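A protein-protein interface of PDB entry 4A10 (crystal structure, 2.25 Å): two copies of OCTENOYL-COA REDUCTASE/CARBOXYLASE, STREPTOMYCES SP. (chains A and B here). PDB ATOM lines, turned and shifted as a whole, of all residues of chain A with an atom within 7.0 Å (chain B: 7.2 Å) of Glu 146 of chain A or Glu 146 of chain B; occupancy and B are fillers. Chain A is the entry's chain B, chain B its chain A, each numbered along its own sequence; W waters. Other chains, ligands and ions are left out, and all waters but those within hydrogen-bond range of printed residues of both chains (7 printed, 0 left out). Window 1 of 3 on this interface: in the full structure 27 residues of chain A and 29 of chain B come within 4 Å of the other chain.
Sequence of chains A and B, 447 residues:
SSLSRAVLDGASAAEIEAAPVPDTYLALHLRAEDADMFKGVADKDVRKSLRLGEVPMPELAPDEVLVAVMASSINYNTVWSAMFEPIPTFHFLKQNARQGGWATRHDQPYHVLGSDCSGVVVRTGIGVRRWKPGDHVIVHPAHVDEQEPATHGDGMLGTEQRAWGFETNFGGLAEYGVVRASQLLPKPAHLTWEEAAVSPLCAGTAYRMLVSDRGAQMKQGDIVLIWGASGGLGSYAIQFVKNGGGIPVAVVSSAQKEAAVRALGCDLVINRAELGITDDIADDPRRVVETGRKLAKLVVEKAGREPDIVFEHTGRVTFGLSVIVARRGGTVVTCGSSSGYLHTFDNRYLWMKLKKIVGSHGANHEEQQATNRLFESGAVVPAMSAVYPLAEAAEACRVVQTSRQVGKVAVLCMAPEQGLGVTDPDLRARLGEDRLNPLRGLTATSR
The side-chain carboxylate of Asp 63 of chain B lies within salt-bridge range of the guanidinium group of Arg 129 of chain A (3.6 Å).
The guanidinium group of Arg 130 of chain B lies within salt-bridge range of the side-chain carboxylate of Asp 145 of chain A (3.7 Å).
The guanidinium group (NE) of Arg 129 of chain B is in salt-bridge range of the side-chain carboxylate (OD2) of Asp 145 of chain A (2.9 Å).
The side-chain carboxylate of Glu 146 of chain A is in salt-bridge range of the guanidinium group of Arg 129 of chain B.
OD1 of Asp 145 of chain B is in salt-bridge range of NE of Arg 129 of chain A (3.2 Å).
A ring nitrogen (NE2) of His 365 of chain A sits at hydrogen-bond distance from the backbone carbonyl oxygen of Gln 147 of chain B, 3.2 Å away.
The backbone carbonyl oxygen of Gln 147 of chain A is in hydrogen-bond range of a ring nitrogen (NE2) of His 365 of chain B, 3.2 Å away.
The backbone NH of Arg 129 of chain B is in hydrogen-bond range of the side-chain amide oxygen of Gln 147 of chain A (2.7 Å).
N of Arg 129 of chain A is in hydrogen-bond range of OE1 of Gln 147 of chain B.
The side-chain carboxylate (OE1) of Glu 146 of chain B is in salt-bridge range of the guanidinium group (NH2) of Arg 129 of chain A (3.0 Å).
The backbone carbonyl oxygen (O) of Ser 182 of chain B is in hydrogen-bond range of a ring nitrogen (ND1) of His 365 of chain B (3.2 Å).
Glu 146 of chain A touches just these residues of chain B: Arg 129 (3.1 Å), Glu 146 (3.4 Å) and Ser 182 (3.8 Å).
Of the printed residues of chain B, Ser 182 of chain A touches Glu 146 and His 152.
Of the printed residues of chain A, Asp 63 of chain B touches Arg 129.
Glu 146 of chain B touches three residues of chain A.
Printed residues of chain A within 4 Å of Pro 149 of chain B: His 365 (3.6 Å).
The nearest residue of chain B that does not touch Glu 146 of chain A is His 152 of chain B (4.1 Å).
Of the 17 printed residues of chain A, 11 touch a printed residue of chain B.
Printed residues of chain A that touch a printed residue of chain B: Arg 129, Val 144, Asp 145, Glu 146, Gln 147, Pro 149, Thr 151, His 152, Ala 181, Ser 182 and His 365.
Along chain A the printed residues that touch a printed residue of chain B span positions 129 to 365.
Hydrophobic or aromatic side chains of chain B within 4 Å of the printed part of chain A: Val 144, Pro 149, His 152, Ala 181 and His 365.
Arg 129 of chain A touches Arg 180 of chain B, but with the chains exchanged Arg 180 of chain A does not touch Arg 129 of chain B (4.1 Å).
Water W2 bridges a ring nitrogen (ND1) of His 152 of chain B and the backbone NH of His 365 of chain A.
Water W4 lies within hydrogen-bond range of NE2 of His 365 of chain B (3.1 Å) and O of Gln 147 of chain A (3.2 Å).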
ATOM      1  N   ASP A  63     -14.826  24.838  12.105  1.00  0.00           N
ATOM      2  CA  ASP A  63     -14.699  25.886  13.118  1.00  0.00           C
ATOM      3  C   ASP A  63     -13.781  27.036  12.610  1.00  0.00           C
ATOM      4  O   ASP A  63     -13.295  27.877  13.386  1.00  0.00           O
ATOM      5  CB  ASP A  63     -14.159  25.255  14.403  1.00  0.00           C
ATOM      6  CG  ASP A  63     -12.680  24.854  14.294  1.00  0.00           C
ATOM      7  OD1 ASP A  63     -12.255  24.270  13.268  1.00  0.00           O
ATOM      8  OD2 ASP A  63     -11.917  25.138  15.250  1.00  0.00           O
ATOM      9  N   ARG A 129     -20.240  30.195  14.799  1.00  0.00           N
ATOM     10  CA  ARG A 129     -21.390  30.955  15.292  1.00  0.00           C
ATOM     11  C   ARG A 129     -21.230  32.461  15.047  1.00  0.00           C
ATOM     12  O   ARG A 129     -20.121  32.977  15.134  1.00  0.00           O
ATOM     13  CB  ARG A 129     -21.598  30.686  16.794  1.00  0.00           C
ATOM     14  CG  ARG A 129     -21.937  29.227  17.133  1.00  0.00           C
ATOM     15  CD  ARG A 129     -22.193  29.039  18.627  1.00  0.00           C
ATOM     16  NE  ARG A 129     -21.017  28.555  19.337  1.00  0.00           N
ATOM     17  CZ  ARG A 129     -20.672  27.270  19.422  1.00  0.00           C
ATOM     18  NH1 ARG A 129     -21.417  26.329  18.842  1.00  0.00           N
ATOM     19  NH2 ARG A 129     -19.583  26.915  20.080  1.00  0.00           N
ATOM     20  N   ALA A 142      -3.511  33.605  18.868  1.00  0.00           N
ATOM     21  CA  ALA A 142      -3.723  32.406  19.681  1.00  0.00           C
ATOM     22  C   ALA A 142      -4.628  31.357  19.014  1.00  0.00           C
ATOM     23  O   ALA A 142      -5.854  31.453  19.053  1.00  0.00           O
ATOM     24  CB  ALA A 142      -4.214  32.772  21.088  1.00  0.00           C
ATOM     25  N   HIS A 143      -3.987  30.374  18.392  1.00  0.00           N
ATOM     26  CA  HIS A 143      -4.615  29.285  17.649  1.00  0.00           C
ATOM     27  C   HIS A 143      -4.628  28.090  18.603  1.00  0.00           C
ATOM     28  O   HIS A 143      -3.595  27.447  18.822  1.00  0.00           O
ATOM     29  CB  HIS A 143      -3.741  28.995  16.424  1.00  0.00           C
ATOM     30  CG  HIS A 143      -4.330  28.021  15.445  1.00  0.00           C
ATOM     31  ND1 HIS A 143      -4.423  26.671  15.698  1.00  0.00           N
ATOM     32  CD2 HIS A 143      -4.787  28.201  14.183  1.00  0.00           C
ATOM     33  CE1 HIS A 143      -4.946  26.062  14.646  1.00  0.00           C
ATOM     34  NE2 HIS A 143      -5.166  26.967  13.709  1.00  0.00           N
ATOM     35  N   VAL A 144      -5.790  27.817  19.188  1.00  0.00           N
ATOM     36  CA  VAL A 144      -5.879  26.921  20.327  1.00  0.00           C
ATOM     37  C   VAL A 144      -6.944  25.872  20.093  1.00  0.00           C
ATOM     38  O   VAL A 144      -7.805  26.025  19.222  1.00  0.00           O
ATOM     39  CB  VAL A 144      -6.148  27.676  21.694  1.00  0.00           C
ATOM     40  CG1 VAL A 144      -5.196  28.875  21.904  1.00  0.00           C
ATOM     41  CG2 VAL A 144      -7.611  28.121  21.836  1.00  0.00           C
ATOM     42  N   ASP A 145      -6.869  24.812  20.898  1.00  0.00           N
ATOM     43  CA  ASP A 145      -7.830  23.713  20.905  1.00  0.00           C
ATOM     44  C   ASP A 145      -8.846  23.891  22.040  1.00  0.00           C
ATOM     45  O   ASP A 145      -8.556  23.633  23.210  1.00  0.00           O
ATOM     46  CB  ASP A 145      -7.071  22.403  21.105  1.00  0.00           C
ATOM     47  CG  ASP A 145      -7.876  21.199  20.741  1.00  0.00           C
ATOM     48  OD1 ASP A 145      -9.026  21.046  21.204  1.00  0.00           O
ATOM     49  OD2 ASP A 145      -7.335  20.381  19.973  1.00  0.00           O
ATOM     50  N   GLU A 146     -10.058  24.279  21.664  1.00  0.00           N
ATOM     51  CA  GLU A 146     -11.156  24.544  22.588  1.00  0.00           C
ATOM     52  C   GLU A 146     -11.752  23.266  23.181  1.00  0.00           C
ATOM     53  O   GLU A 146     -12.657  23.316  24.023  1.00  0.00           O
ATOM     54  CB  GLU A 146     -12.243  25.319  21.840  1.00  0.00           C
ATOM     55  CG  GLU A 146     -11.752  26.580  21.106  1.00  0.00           C
ATOM     56  CD  GLU A 146     -11.086  26.302  19.755  1.00  0.00           C
ATOM     57  OE1 GLU A 146     -10.820  25.119  19.412  1.00  0.00           O
ATOM     58  OE2 GLU A 146     -10.808  27.289  19.029  1.00  0.00           O
ATOM     59  N   GLN A 147     -11.232  22.118  22.764  1.00  0.00           N
ATOM     60  CA  GLN A 147     -11.660  20.847  23.329  1.00  0.00           C
ATOM     61  C   GLN A 147     -10.826  20.395  24.532  1.00  0.00           C
ATOM     62  O   GLN A 147     -11.297  19.610  25.366  1.00  0.00           O
ATOM     63  CB  GLN A 147     -11.609  19.764  22.273  1.00  0.00           C
ATOM     64  CG  GLN A 147     -12.923  19.431  21.659  1.00  0.00           C
ATOM     65  CD  GLN A 147     -12.822  18.187  20.775  1.00  0.00           C
ATOM     66  OE1 GLN A 147     -12.880  18.296  19.562  1.00  0.00           O
ATOM     67  NE2 GLN A 147     -12.638  17.012  21.391  1.00  0.00           N
ATOM     68  N   GLU A 148      -9.582  20.855  24.568  1.00  0.00           N
ATOM     69  CA  GLU A 148      -8.633  20.612  25.638  1.00  0.00           C
ATOM     70  C   GLU A 148      -9.088  21.257  26.966  1.00  0.00           C
ATOM     71  O   GLU A 148      -9.449  22.424  26.987  1.00  0.00           O
ATOM     72  CB  GLU A 148      -7.295  21.247  25.227  1.00  0.00           C
ATOM     73  CG  GLU A 148      -6.104  20.325  25.236  1.00  0.00           C
ATOM     74  CD  GLU A 148      -4.770  21.077  25.221  1.00  0.00           C
ATOM     75  OE1 GLU A 148      -4.571  21.970  24.368  1.00  0.00           O
ATOM     76  OE2 GLU A 148      -3.916  20.772  26.078  1.00  0.00           O
ATOM     77  N   PRO A 149      -9.057  20.504  28.081  1.00  0.00           N
ATOM     78  CA  PRO A 149      -9.487  21.080  29.364  1.00  0.00           C
ATOM     79  C   PRO A 149      -8.724  22.355  29.828  1.00  0.00           C
ATOM     80  O   PRO A 149      -9.355  23.292  30.324  1.00  0.00           O
ATOM     81  CB  PRO A 149      -9.281  19.923  30.338  1.00  0.00           C
ATOM     82  CG  PRO A 149      -9.559  18.709  29.509  1.00  0.00           C
ATOM     83  CD  PRO A 149      -8.979  19.028  28.145  1.00  0.00           C
ATOM     84  N   THR A 151      -7.468  24.857  28.118  1.00  0.00           N
ATOM     85  CA  THR A 151      -8.019  26.020  27.407  1.00  0.00           C
ATOM     86  C   THR A 151      -9.118  26.767  28.195  1.00  0.00           C
ATOM     87  O   THR A 151      -9.209  28.005  28.122  1.00  0.00           O
ATOM     88  CB  THR A 151      -8.510  25.616  26.000  1.00  0.00           C
ATOM     89  OG1 THR A 151      -7.408  25.078  25.253  1.00  0.00           O
ATOM     90  CG2 THR A 151      -9.095  26.814  25.232  1.00  0.00           C
ATOM     91  N   HIS A 152      -9.932  26.012  28.942  1.00  0.00           N
ATOM     92  CA  HIS A 152     -11.045  26.555  29.741  1.00  0.00           C
ATOM     93  C   HIS A 152     -10.643  27.132  31.106  1.00  0.00           C
ATOM     94  O   HIS A 152     -11.503  27.555  31.909  1.00  0.00           O
ATOM     95  CB  HIS A 152     -12.107  25.481  29.934  1.00  0.00           C
ATOM     96  CG  HIS A 152     -12.709  25.002  28.651  1.00  0.00           C
ATOM     97  ND1 HIS A 152     -13.964  25.380  28.231  1.00  0.00           N
ATOM     98  CD2 HIS A 152     -12.216  24.194  27.683  1.00  0.00           C
ATOM     99  CE1 HIS A 152     -14.231  24.804  27.072  1.00  0.00           C
ATOM    100  NE2 HIS A 152     -13.186  24.082  26.713  1.00  0.00           N
ATOM    101  N   ARG A 180      -9.080  30.083  13.140  1.00  0.00           N
ATOM    102  CA  ARG A 180     -10.163  29.590  13.981  1.00  0.00           C
ATOM    103  C   ARG A 180     -11.034  30.761  14.372  1.00  0.00           C
ATOM    104  O   ARG A 180     -10.541  31.886  14.553  1.00  0.00           O
ATOM    105  CB  ARG A 180      -9.670  28.893  15.246  1.00  0.00           C
ATOM    106  CG  ARG A 180      -8.907  27.635  14.990  1.00  0.00           C
ATOM    107  CD  ARG A 180      -9.026  26.676  16.155  1.00  0.00           C
ATOM    108  NE  ARG A 180      -8.758  25.321  15.693  1.00  0.00           N
ATOM    109  CZ  ARG A 180      -7.715  24.594  16.092  1.00  0.00           C
ATOM    110  NH1 ARG A 180      -6.852  25.094  16.973  1.00  0.00           N
ATOM    111  NH2 ARG A 180      -7.533  23.369  15.604  1.00  0.00           N
ATOM    112  N   ALA A 181     -12.327  30.478  14.509  1.00  0.00           N
ATOM    113  CA  ALA A 181     -13.304  31.463  14.939  1.00  0.00           C
ATOM    114  C   ALA A 181     -12.935  32.124  16.275  1.00  0.00           C
ATOM    115  O   ALA A 181     -13.287  33.288  16.514  1.00  0.00           O
ATOM    116  CB  ALA A 181     -14.690  30.828  15.005  1.00  0.00           C
ATOM    117  N   SER A 182     -12.209  31.401  17.127  1.00  0.00           N
ATOM    118  CA  SER A 182     -11.765  31.954  18.401  1.00  0.00           C
ATOM    119  C   SER A 182     -10.469  32.777  18.293  1.00  0.00           C
ATOM    120  O   SER A 182      -9.887  33.134  19.305  1.00  0.00           O
ATOM    121  CB  SER A 182     -11.626  30.855  19.462  1.00  0.00           C
ATOM    122  OG  SER A 182     -10.742  29.837  19.020  1.00  0.00           O
ATOM    123  N   GLN A 183     -10.034  33.086  17.071  1.00  0.00           N
ATOM    124  CA  GLN A 183      -8.998  34.110  16.872  1.00  0.00           C
ATOM    125  C   GLN A 183      -9.597  35.473  16.460  1.00  0.00           C
ATOM    126  O   GLN A 183      -8.875  36.434  16.295  1.00  0.00           O
ATOM    127  CB  GLN A 183      -8.018  33.696  15.784  1.00  0.00           C
ATOM    128  CG  GLN A 183      -7.170  32.482  16.059  1.00  0.00           C
ATOM    129  CD  GLN A 183      -6.371  32.104  14.828  1.00  0.00           C
ATOM    130  OE1 GLN A 183      -6.676  31.125  14.163  1.00  0.00           O
ATOM    131  NE2 GLN A 183      -5.375  32.918  14.494  1.00  0.00           N
ATOM    132  N   HIS A 365      -7.953  34.543  24.233  1.00  0.00           N
ATOM    133  CA  HIS A 365      -9.066  35.233  23.603  1.00  0.00           C
ATOM    134  C   HIS A 365      -9.763  36.257  24.530  1.00  0.00           C
ATOM    135  O   HIS A 365     -10.227  37.287  24.053  1.00  0.00           O
ATOM    136  CB  HIS A 365     -10.039  34.178  23.065  1.00  0.00           C
ATOM    137  CG  HIS A 365     -10.986  34.664  22.011  1.00  0.00           C
ATOM    138  ND1 HIS A 365     -10.685  35.682  21.126  1.00  0.00           N
ATOM    139  CD2 HIS A 365     -12.215  34.210  21.655  1.00  0.00           C
ATOM    140  CE1 HIS A 365     -11.707  35.868  20.310  1.00  0.00           C
ATOM    141  NE2 HIS A 365     -12.640  34.979  20.600  1.00  0.00           N
ATOM    142  N   ASP B  63     -19.662  20.157  16.353  1.00  0.00           N
ATOM    143  CA  ASP B  63     -18.804  20.075  17.541  1.00  0.00           C
ATOM    144  C   ASP B  63     -19.450  19.201  18.625  1.00  0.00           C
ATOM    145  O   ASP B  63     -19.056  19.238  19.802  1.00  0.00           O
ATOM    146  CB  ASP B  63     -18.472  21.477  18.069  1.00  0.00           C
ATOM    147  CG  ASP B  63     -19.723  22.283  18.468  1.00  0.00           C
ATOM    148  OD1 ASP B  63     -20.835  22.021  17.940  1.00  0.00           O
ATOM    149  OD2 ASP B  63     -19.606  23.203  19.329  1.00  0.00           O
ATOM    150  N   ARG B 129     -12.417  16.463  17.587  1.00  0.00           N
ATOM    151  CA  ARG B 129     -11.064  15.934  17.610  1.00  0.00           C
ATOM    152  C   ARG B 129     -10.952  14.747  18.570  1.00  0.00           C
ATOM    153  O   ARG B 129     -11.624  14.712  19.604  1.00  0.00           O
ATOM    154  CB  ARG B 129     -10.079  17.049  17.994  1.00  0.00           C
ATOM    155  CG  ARG B 129     -10.051  18.187  16.972  1.00  0.00           C
ATOM    156  CD  ARG B 129      -8.998  19.243  17.256  1.00  0.00           C
ATOM    157  NE  ARG B 129      -9.511  20.299  18.118  1.00  0.00           N
ATOM    158  CZ  ARG B 129     -10.424  21.197  17.739  1.00  0.00           C
ATOM    159  NH1 ARG B 129     -10.929  21.168  16.501  1.00  0.00           N
ATOM    160  NH2 ARG B 129     -10.839  22.121  18.594  1.00  0.00           N
ATOM    161  N   ARG B 130     -10.134  13.766  18.185  1.00  0.00           N
ATOM    162  CA  ARG B 130      -9.720  12.621  19.030  1.00  0.00           C
ATOM    163  C   ARG B 130     -10.761  11.554  19.389  1.00  0.00           C
ATOM    164  O   ARG B 130     -10.493  10.352  19.233  1.00  0.00           O
ATOM    165  CB  ARG B 130      -9.032  13.103  20.306  1.00  0.00           C
ATOM    166  CG  ARG B 130      -7.785  13.923  20.027  1.00  0.00           C
ATOM    167  CD  ARG B 130      -7.409  14.759  21.227  1.00  0.00           C
ATOM    168  NE  ARG B 130      -6.852  16.012  20.743  1.00  0.00           N
ATOM    169  CZ  ARG B 130      -7.316  17.228  21.022  1.00  0.00           C
ATOM    170  NH1 ARG B 130      -8.342  17.410  21.853  1.00  0.00           N
ATOM    171  NH2 ARG B 130      -6.706  18.273  20.483  1.00  0.00           N
ATOM    172  N   ALA B 142     -21.140  21.440  31.978  1.00  0.00           N
ATOM    173  CA  ALA B 142     -20.792  22.773  31.473  1.00  0.00           C
ATOM    174  C   ALA B 142     -20.885  22.839  29.930  1.00  0.00           C
ATOM    175  O   ALA B 142     -19.971  22.398  29.225  1.00  0.00           O
ATOM    176  CB  ALA B 142     -19.407  23.201  31.960  1.00  0.00           C
ATOM    177  N   HIS B 143     -22.001  23.383  29.446  1.00  0.00           N
ATOM    178  CA  HIS B 143     -22.345  23.462  28.027  1.00  0.00           C
ATOM    179  C   HIS B 143     -22.123  24.928  27.639  1.00  0.00           C
ATOM    180  O   HIS B 143     -22.920  25.813  27.974  1.00  0.00           O
ATOM    181  CB  HIS B 143     -23.803  22.982  27.818  1.00  0.00           C
ATOM    182  CG  HIS B 143     -24.259  22.927  26.384  1.00  0.00           C
ATOM    183  ND1 HIS B 143     -24.755  24.026  25.720  1.00  0.00           N
ATOM    184  CD2 HIS B 143     -24.366  21.888  25.518  1.00  0.00           C
ATOM    185  CE1 HIS B 143     -25.116  23.681  24.497  1.00  0.00           C
ATOM    186  NE2 HIS B 143     -24.887  22.388  24.345  1.00  0.00           N
ATOM    187  N   VAL B 144     -21.005  25.160  26.959  1.00  0.00           N
ATOM    188  CA  VAL B 144     -20.419  26.484  26.828  1.00  0.00           C
ATOM    189  C   VAL B 144     -20.041  26.767  25.385  1.00  0.00           C
ATOM    190  O   VAL B 144     -19.910  25.848  24.564  1.00  0.00           O
ATOM    191  CB  VAL B 144     -19.151  26.649  27.730  1.00  0.00           C
ATOM    192  CG1 VAL B 144     -19.440  26.243  29.179  1.00  0.00           C
ATOM    193  CG2 VAL B 144     -17.948  25.861  27.166  1.00  0.00           C
ATOM    194  N   ASP B 145     -19.848  28.049  25.096  1.00  0.00           N
ATOM    195  CA  ASP B 145     -19.533  28.514  23.753  1.00  0.00           C
ATOM    196  C   ASP B 145     -18.056  28.849  23.668  1.00  0.00           C
ATOM    197  O   ASP B 145     -17.608  29.880  24.178  1.00  0.00           O
ATOM    198  CB  ASP B 145     -20.368  29.747  23.415  1.00  0.00           C
ATOM    199  CG  ASP B 145     -20.107  30.263  22.034  1.00  0.00           C
ATOM    200  OD1 ASP B 145     -19.072  29.926  21.415  1.00  0.00           O
ATOM    201  OD2 ASP B 145     -20.961  31.022  21.550  1.00  0.00           O
ATOM    202  N   GLU B 146     -17.323  27.992  22.961  1.00  0.00           N
ATOM    203  CA  GLU B 146     -15.871  28.050  22.920  1.00  0.00           C
ATOM    204  C   GLU B 146     -15.366  29.198  22.042  1.00  0.00           C
ATOM    205  O   GLU B 146     -14.154  29.475  21.993  1.00  0.00           O
ATOM    206  CB  GLU B 146     -15.314  26.711  22.426  1.00  0.00           C
ATOM    207  CG  GLU B 146     -15.704  25.511  23.288  1.00  0.00           C
ATOM    208  CD  GLU B 146     -17.073  24.957  22.932  1.00  0.00           C
ATOM    209  OE1 GLU B 146     -17.822  25.621  22.158  1.00  0.00           O
ATOM    210  OE2 GLU B 146     -17.393  23.837  23.417  1.00  0.00           O
ATOM    211  N   GLN B 147     -16.298  29.889  21.397  1.00  0.00           N
ATOM    212  CA  GLN B 147     -16.001  31.056  20.559  1.00  0.00           C
ATOM    213  C   GLN B 147     -15.959  32.361  21.331  1.00  0.00           C
ATOM    214  O   GLN B 147     -15.306  33.313  20.922  1.00  0.00           O
ATOM    215  CB  GLN B 147     -17.035  31.203  19.455  1.00  0.00           C
ATOM    216  CG  GLN B 147     -16.482  30.967  18.083  1.00  0.00           C
ATOM    217  CD  GLN B 147     -17.482  31.302  17.003  1.00  0.00           C
ATOM    218  OE1 GLN B 147     -18.059  30.409  16.391  1.00  0.00           O
ATOM    219  NE2 GLN B 147     -17.702  32.592  16.770  1.00  0.00           N
ATOM    220  N   GLU B 148     -16.695  32.400  22.437  1.00  0.00           N
ATOM    221  CA  GLU B 148     -16.744  33.531  23.369  1.00  0.00           C
ATOM    222  C   GLU B 148     -15.398  33.801  24.059  1.00  0.00           C
ATOM    223  O   GLU B 148     -14.800  32.882  24.616  1.00  0.00           O
ATOM    224  CB  GLU B 148     -17.743  33.223  24.482  1.00  0.00           C
ATOM    225  CG  GLU B 148     -19.151  33.745  24.297  1.00  0.00           C
ATOM    226  CD  GLU B 148     -19.926  33.760  25.617  1.00  0.00           C
ATOM    227  OE1 GLU B 148     -20.434  32.704  26.030  1.00  0.00           O
ATOM    228  OE2 GLU B 148     -20.018  34.834  26.243  1.00  0.00           O
ATOM    229  N   PRO B 149     -14.942  35.067  24.069  1.00  0.00           N
ATOM    230  CA  PRO B 149     -13.712  35.389  24.799  1.00  0.00           C
ATOM    231  C   PRO B 149     -13.686  34.874  26.234  1.00  0.00           C
ATOM    232  O   PRO B 149     -12.723  34.213  26.611  1.00  0.00           O
ATOM    233  CB  PRO B 149     -13.684  36.910  24.790  1.00  0.00           C
ATOM    234  CG  PRO B 149     -14.335  37.247  23.466  1.00  0.00           C
ATOM    235  CD  PRO B 149     -15.438  36.222  23.296  1.00  0.00           C
ATOM    236  N   THR B 151     -14.858  32.503  27.863  1.00  0.00           N
ATOM    237  CA  THR B 151     -14.582  31.057  27.977  1.00  0.00           C
ATOM    238  C   THR B 151     -13.092  30.681  28.095  1.00  0.00           C
ATOM    239  O   THR B 151     -12.766  29.684  28.726  1.00  0.00           O
ATOM    240  CB  THR B 151     -15.243  30.231  26.799  1.00  0.00           C
ATOM    241  OG1 THR B 151     -16.640  30.517  26.740  1.00  0.00           O
ATOM    242  CG2 THR B 151     -15.073  28.712  26.999  1.00  0.00           C
ATOM    243  N   HIS B 152     -12.220  31.476  27.471  1.00  0.00           N
ATOM    244  CA  HIS B 152     -10.780  31.236  27.435  1.00  0.00           C
ATOM    245  C   HIS B 152     -10.068  31.830  28.650  1.00  0.00           C
ATOM    246  O   HIS B 152      -8.843  31.759  28.772  1.00  0.00           O
ATOM    247  CB  HIS B 152     -10.198  31.813  26.138  1.00  0.00           C
ATOM    248  CG  HIS B 152     -10.719  31.145  24.901  1.00  0.00           C
ATOM    249  ND1 HIS B 152      -9.911  30.438  24.039  1.00  0.00           N
ATOM    250  CD2 HIS B 152     -11.972  31.062  24.393  1.00  0.00           C
ATOM    251  CE1 HIS B 152     -10.639  29.958  23.045  1.00  0.00           C
ATOM    252  NE2 HIS B 152     -11.895  30.317  23.240  1.00  0.00           N
ATOM    253  N   ARG B 180     -21.737  18.676  23.703  1.00  0.00           N
ATOM    254  CA  ARG B 180     -20.555  19.290  23.102  1.00  0.00           C
ATOM    255  C   ARG B 180     -19.337  18.499  23.521  1.00  0.00           C
ATOM    256  O   ARG B 180     -19.291  17.962  24.629  1.00  0.00           O
ATOM    257  CB  ARG B 180     -20.390  20.762  23.521  1.00  0.00           C
ATOM    258  CG  ARG B 180     -21.444  21.672  22.925  1.00  0.00           C
ATOM    259  CD  ARG B 180     -21.175  23.170  23.078  1.00  0.00           C
ATOM    260  NE  ARG B 180     -22.153  23.841  22.233  1.00  0.00           N
ATOM    261  CZ  ARG B 180     -22.529  25.116  22.313  1.00  0.00           C
ATOM    262  NH1 ARG B 180     -21.987  25.934  23.195  1.00  0.00           N
ATOM    263  NH2 ARG B 180     -23.463  25.571  21.480  1.00  0.00           N
ATOM    264  N   ALA B 181     -18.342  18.448  22.644  1.00  0.00           N
ATOM    265  CA  ALA B 181     -17.115  17.692  22.910  1.00  0.00           C
ATOM    266  C   ALA B 181     -16.335  18.232  24.110  1.00  0.00           C
ATOM    267  O   ALA B 181     -15.590  17.496  24.760  1.00  0.00           O
ATOM    268  CB  ALA B 181     -16.241  17.635  21.677  1.00  0.00           C
ATOM    269  N   SER B 182     -16.519  19.512  24.414  1.00  0.00           N
ATOM    270  CA  SER B 182     -15.910  20.089  25.603  1.00  0.00           C
ATOM    271  C   SER B 182     -16.675  19.757  26.902  1.00  0.00           C
ATOM    272  O   SER B 182     -16.411  20.356  27.944  1.00  0.00           O
ATOM    273  CB  SER B 182     -15.765  21.593  25.430  1.00  0.00           C
ATOM    274  OG  SER B 182     -17.032  22.171  25.200  1.00  0.00           O
ATOM    275  N   GLN B 183     -17.620  18.818  26.818  1.00  0.00           N
ATOM    276  CA  GLN B 183     -18.250  18.220  28.012  1.00  0.00           C
ATOM    277  C   GLN B 183     -17.698  16.824  28.338  1.00  0.00           C
ATOM    278  O   GLN B 183     -18.056  16.243  29.353  1.00  0.00           O
ATOM    279  CB  GLN B 183     -19.755  18.081  27.815  1.00  0.00           C
ATOM    280  CG  GLN B 183     -20.512  19.375  27.749  1.00  0.00           C
ATOM    281  CD  GLN B 183     -21.976  19.141  27.499  1.00  0.00           C
ATOM    282  OE1 GLN B 183     -22.477  19.406  26.412  1.00  0.00           O
ATOM    283  NE2 GLN B 183     -22.672  18.628  28.507  1.00  0.00           N
ATOM    284  N   HIS B 365     -14.349  23.060  32.253  1.00  0.00           N
ATOM    285  CA  HIS B 365     -13.697  21.858  31.705  1.00  0.00           C
ATOM    286  C   HIS B 365     -12.330  21.546  32.366  1.00  0.00           C
ATOM    287  O   HIS B 365     -11.989  20.377  32.558  1.00  0.00           O
ATOM    288  CB  HIS B 365     -13.563  22.006  30.184  1.00  0.00           C
ATOM    289  CG  HIS B 365     -13.423  20.718  29.432  1.00  0.00           C
ATOM    290  ND1 HIS B 365     -14.020  19.542  29.835  1.00  0.00           N
ATOM    291  CD2 HIS B 365     -12.816  20.446  28.252  1.00  0.00           C
ATOM    292  CE1 HIS B 365     -13.735  18.590  28.963  1.00  0.00           C
ATOM    293  NE2 HIS B 365     -13.010  19.113  27.993  1.00  0.00           N
HETATM  294  O   HOH W   1     -12.940  16.697  24.166  1.00  0.00           O
HETATM  295  O   HOH W   2      -7.360  31.703  23.744  1.00  0.00           O
HETATM  296  O   HOH W   3     -17.423  24.945  18.679  1.00  0.00           O
HETATM  297  O   HOH W   4     -11.719  16.688  26.648  1.00  0.00           O
HETATM  298  O   HOH W   5      -9.398  17.165  24.601  1.00  0.00           O
HETATM  299  O   HOH W   6     -15.011  34.809  17.892  1.00  0.00           O
HETATM  300  O   HOH W   7     -15.788  24.864  30.474  1.00  0.00           O
